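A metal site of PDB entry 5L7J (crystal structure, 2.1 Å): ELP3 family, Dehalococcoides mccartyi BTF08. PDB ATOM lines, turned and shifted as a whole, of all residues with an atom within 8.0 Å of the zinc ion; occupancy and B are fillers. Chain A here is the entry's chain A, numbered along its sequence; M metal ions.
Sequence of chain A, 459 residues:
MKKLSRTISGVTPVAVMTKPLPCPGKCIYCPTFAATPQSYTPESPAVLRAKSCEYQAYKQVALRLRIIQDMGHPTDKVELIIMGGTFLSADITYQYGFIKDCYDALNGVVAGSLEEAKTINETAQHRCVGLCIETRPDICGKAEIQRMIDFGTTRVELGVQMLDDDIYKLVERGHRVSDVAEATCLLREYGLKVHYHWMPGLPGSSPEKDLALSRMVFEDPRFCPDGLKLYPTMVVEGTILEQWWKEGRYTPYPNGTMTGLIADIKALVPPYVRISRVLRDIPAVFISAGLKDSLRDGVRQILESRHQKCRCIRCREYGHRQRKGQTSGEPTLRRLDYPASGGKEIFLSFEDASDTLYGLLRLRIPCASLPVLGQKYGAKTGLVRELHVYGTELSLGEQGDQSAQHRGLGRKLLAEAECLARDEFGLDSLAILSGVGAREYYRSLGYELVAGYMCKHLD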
ATOM      1  N   LYS A 266      24.447  17.319  25.376  1.00  0.00           N
ATOM      2  CA  LYS A 266      23.246  16.730  24.792  1.00  0.00           C
ATOM      3  C   LYS A 266      22.973  15.327  25.330  1.00  0.00           C
ATOM      4  O   LYS A 266      21.831  14.888  25.381  1.00  0.00           O
ATOM      5  CB  LYS A 266      23.358  16.677  23.269  1.00  0.00           C
ATOM      6  CG  LYS A 266      23.271  18.022  22.568  1.00  0.00           C
ATOM      7  CD  LYS A 266      23.169  17.847  21.064  1.00  0.00           C
ATOM      8  CE  LYS A 266      22.957  19.172  20.356  1.00  0.00           C
ATOM      9  NZ  LYS A 266      22.770  18.985  18.886  1.00  0.00           N
ATOM     10  N   VAL A 269      20.713  15.239  28.914  1.00  0.00           N
ATOM     11  CA  VAL A 269      19.482  15.987  29.082  1.00  0.00           C
ATOM     12  C   VAL A 269      18.279  15.072  29.315  1.00  0.00           C
ATOM     13  O   VAL A 269      18.140  14.025  28.667  1.00  0.00           O
ATOM     14  CB  VAL A 269      19.194  16.907  27.878  1.00  0.00           C
ATOM     15  CG1 VAL A 269      20.266  17.976  27.784  1.00  0.00           C
ATOM     16  CG2 VAL A 269      19.132  16.095  26.590  1.00  0.00           C
ATOM     17  N   VAL A 273      13.331  17.977  28.098  1.00  0.00           N
ATOM     18  CA  VAL A 273      14.147  19.103  27.663  1.00  0.00           C
ATOM     19  C   VAL A 273      14.284  19.159  26.148  1.00  0.00           C
ATOM     20  O   VAL A 273      14.495  18.129  25.502  1.00  0.00           O
ATOM     21  CB  VAL A 273      15.546  19.047  28.311  1.00  0.00           C
ATOM     22  CG1 VAL A 273      16.435  20.177  27.799  1.00  0.00           C
ATOM     23  CG2 VAL A 273      15.434  19.110  29.825  1.00  0.00           C
ATOM     24  N   ARG A 274      14.174  20.352  25.576  1.00  0.00           N
ATOM     25  CA  ARG A 274      14.358  20.546  24.147  1.00  0.00           C
ATOM     26  C   ARG A 274      15.635  21.348  23.863  1.00  0.00           C
ATOM     27  O   ARG A 274      15.768  22.484  24.308  1.00  0.00           O
ATOM     28  CB  ARG A 274      13.146  21.256  23.537  1.00  0.00           C
ATOM     29  CG  ARG A 274      13.154  21.276  22.017  1.00  0.00           C
ATOM     30  CD  ARG A 274      11.969  22.040  21.460  1.00  0.00           C
ATOM     31  NE  ARG A 274      11.832  21.852  20.019  1.00  0.00           N
ATOM     32  CZ  ARG A 274      12.505  22.542  19.098  1.00  0.00           C
ATOM     33  NH1 ARG A 274      13.367  23.469  19.474  1.00  0.00           N
ATOM     34  NH2 ARG A 274      12.318  22.296  17.811  1.00  0.00           N
ATOM     35  N   ILE A 275      16.561  20.740  23.125  1.00  0.00           N
ATOM     36  CA  ILE A 275      17.815  21.410  22.794  1.00  0.00           C
ATOM     37  C   ILE A 275      17.783  22.008  21.387  1.00  0.00           C
ATOM     38  O   ILE A 275      17.361  21.350  20.436  1.00  0.00           O
ATOM     39  CB  ILE A 275      19.010  20.453  22.885  1.00  0.00           C
ATOM     40  CG1 ILE A 275      19.016  19.715  24.224  1.00  0.00           C
ATOM     41  CG2 ILE A 275      20.320  21.199  22.686  1.00  0.00           C
ATOM     42  CD1 ILE A 275      20.157  18.745  24.346  1.00  0.00           C
ATOM     43  N   SER A 276      18.223  23.254  21.272  1.00  0.00           N
ATOM     44  CA  SER A 276      18.341  23.908  19.971  1.00  0.00           C
ATOM     45  C   SER A 276      19.670  24.644  19.870  1.00  0.00           C
ATOM     46  O   SER A 276      20.118  25.273  20.829  1.00  0.00           O
ATOM     47  CB  SER A 276      17.168  24.860  19.739  1.00  0.00           C
ATOM     48  OG  SER A 276      17.126  25.857  20.745  1.00  0.00           O
ATOM     49  N   ARG A 277      20.302  24.573  18.697  1.00  0.00           N
ATOM     50  CA  ARG A 277      21.573  25.246  18.468  1.00  0.00           C
ATOM     51  C   ARG A 277      21.368  26.519  17.653  1.00  0.00           C
ATOM     52  O   ARG A 277      20.596  26.535  16.692  1.00  0.00           O
ATOM     53  CB  ARG A 277      22.548  24.313  17.745  1.00  0.00           C
ATOM     54  CG  ARG A 277      23.932  24.904  17.545  1.00  0.00           C
ATOM     55  N   LYS A 309      23.948   9.662  20.754  1.00  0.00           N
ATOM     56  CA  LYS A 309      23.113  10.650  20.094  1.00  0.00           C
ATOM     57  C   LYS A 309      22.299  11.452  21.105  1.00  0.00           C
ATOM     58  O   LYS A 309      22.330  11.168  22.303  1.00  0.00           O
ATOM     59  N   CYS A 310      21.577  12.455  20.623  1.00  0.00           N
ATOM     60  CA  CYS A 310      20.757  13.294  21.491  1.00  0.00           C
ATOM     61  C   CYS A 310      19.368  12.697  21.684  1.00  0.00           C
ATOM     62  O   CYS A 310      18.698  12.320  20.720  1.00  0.00           O
ATOM     63  CB  CYS A 310      20.634  14.710  20.910  1.00  0.00           C
ATOM     64  SG  CYS A 310      19.652  15.853  21.909  1.00  0.00           S
ATOM     65  N   ARG A 311      18.935  12.585  22.935  1.00  0.00           N
ATOM     66  CA  ARG A 311      17.633  12.019  23.251  1.00  0.00           C
ATOM     67  C   ARG A 311      16.668  13.086  23.781  1.00  0.00           C
ATOM     68  O   ARG A 311      15.788  12.798  24.587  1.00  0.00           O
ATOM     69  CB  ARG A 311      17.766  10.889  24.265  1.00  0.00           C
ATOM     70  CG  ARG A 311      18.532  11.258  25.525  1.00  0.00           C
ATOM     71  N   CYS A 312      16.851  14.316  23.315  1.00  0.00           N
ATOM     72  CA  CYS A 312      15.987  15.418  23.737  1.00  0.00           C
ATOM     73  C   CYS A 312      14.694  15.430  22.930  1.00  0.00           C
ATOM     74  O   CYS A 312      14.398  14.480  22.209  1.00  0.00           O
ATOM     75  CB  CYS A 312      16.710  16.764  23.595  1.00  0.00           C
ATOM     76  SG  CYS A 312      16.779  17.416  21.904  1.00  0.00           S
ATOM     77  N   ILE A 313      13.936  16.508  23.074  1.00  0.00           N
ATOM     78  CA  ILE A 313      12.647  16.642  22.393  1.00  0.00           C
ATOM     79  C   ILE A 313      12.824  16.834  20.884  1.00  0.00           C
ATOM     80  O   ILE A 313      12.108  16.226  20.087  1.00  0.00           O
ATOM     81  CB  ILE A 313      11.836  17.825  22.976  1.00  0.00           C
ATOM     82  CG1 ILE A 313      11.473  17.543  24.430  1.00  0.00           C
ATOM     83  CG2 ILE A 313      10.582  18.065  22.166  1.00  0.00           C
ATOM     84  CD1 ILE A 313      10.640  18.625  25.069  1.00  0.00           C
ATOM     85  N   ARG A 314      13.778  17.673  20.506  1.00  0.00           N
ATOM     86  CA  ARG A 314      14.031  17.992  19.103  1.00  0.00           C
ATOM     87  C   ARG A 314      14.597  16.792  18.323  1.00  0.00           C
ATOM     88  O   ARG A 314      14.449  16.712  17.102  1.00  0.00           O
ATOM     89  CB  ARG A 314      14.971  19.184  18.985  1.00  0.00           C
ATOM     90  CG  ARG A 314      15.252  19.618  17.554  1.00  0.00           C
ATOM     91  CD  ARG A 314      16.449  20.540  17.463  1.00  0.00           C
ATOM     92  NE  ARG A 314      16.937  20.654  16.089  1.00  0.00           N
ATOM     93  CZ  ARG A 314      18.029  21.323  15.742  1.00  0.00           C
ATOM     94  NH1 ARG A 314      18.397  21.370  14.471  1.00  0.00           N
ATOM     95  NH2 ARG A 314      18.764  21.942  16.663  1.00  0.00           N
ATOM     96  N   CYS A 315      15.235  15.873  19.033  1.00  0.00           N
ATOM     97  CA  CYS A 315      15.807  14.699  18.372  1.00  0.00           C
ATOM     98  C   CYS A 315      14.927  13.463  18.578  1.00  0.00           C
ATOM     99  O   CYS A 315      15.412  12.339  18.670  1.00  0.00           O
ATOM    100  CB  CYS A 315      17.226  14.443  18.889  1.00  0.00           C
ATOM    101  SG  CYS A 315      18.402  15.773  18.493  1.00  0.00           S
ATOM    102  N   ARG A 316      13.617  13.710  18.655  1.00  0.00           N
ATOM    103  CA  ARG A 316      12.618  12.656  18.765  1.00  0.00           C
ATOM    104  C   ARG A 316      11.357  13.051  17.987  1.00  0.00           C
ATOM    105  O   ARG A 316      10.298  12.460  18.160  1.00  0.00           O
ATOM    106  CB  ARG A 316      12.259  12.380  20.226  1.00  0.00           C
ATOM    107  CG  ARG A 316      13.232  11.493  20.990  1.00  0.00           C
ATOM    108  CD  ARG A 316      12.721  11.216  22.402  1.00  0.00           C
ATOM    109  NE  ARG A 316      12.775  12.410  23.253  1.00  0.00           N
ATOM    110  CZ  ARG A 316      11.933  12.666  24.239  1.00  0.00           C
ATOM    111  NH1 ARG A 316      10.949  11.827  24.519  1.00  0.00           N
ATOM    112  NH2 ARG A 316      12.068  13.771  24.957  1.00  0.00           N
ATOM    113  N   GLU A 317      11.514  14.044  17.115  1.00  0.00           N
ATOM    114  CA  GLU A 317      10.401  14.781  16.521  1.00  0.00           C
ATOM    115  C   GLU A 317       9.376  13.998  15.717  1.00  0.00           C
ATOM    116  O   GLU A 317       8.176  14.271  15.820  1.00  0.00           O
ATOM    117  CB  GLU A 317      10.958  15.882  15.613  1.00  0.00           C
ATOM    118  CG  GLU A 317      11.537  17.056  16.359  1.00  0.00           C
ATOM    119  CD  GLU A 317      12.066  18.124  15.425  1.00  0.00           C
ATOM    120  OE1 GLU A 317      12.143  17.862  14.205  1.00  0.00           O
ATOM    121  OE2 GLU A 317      12.409  19.230  15.911  1.00  0.00           O
HETATM  122 ZN    ZN M   1      18.483  17.103  20.374  1.00  0.00          ZN
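The guanidinium group (NE) of Arg 316 sits at hydrogen-bond distance from the backbone carbonyl oxygen (O) of Cys 312, at 2.8 Å.
SG of Cys 312 sits close to N of Ile 275, at 3.5 Å.
The side-chain sulfur of Cys 312 sits close to the backbone NH of Arg 314 (3.3 Å).
Within 4 Å of the zinc ion: Cys 310, Cys 312 and Cys 315.
The zinc ion is bound by the side-chain sulfur (SG) of Cys 310 (2.3 Å), the side-chain sulfur (SG) of Cys 315 (2.3 Å) and the side-chain sulfur (SG) of Cys 312 (2.3 Å).
The zinc ion has three donor atoms within binding distance.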
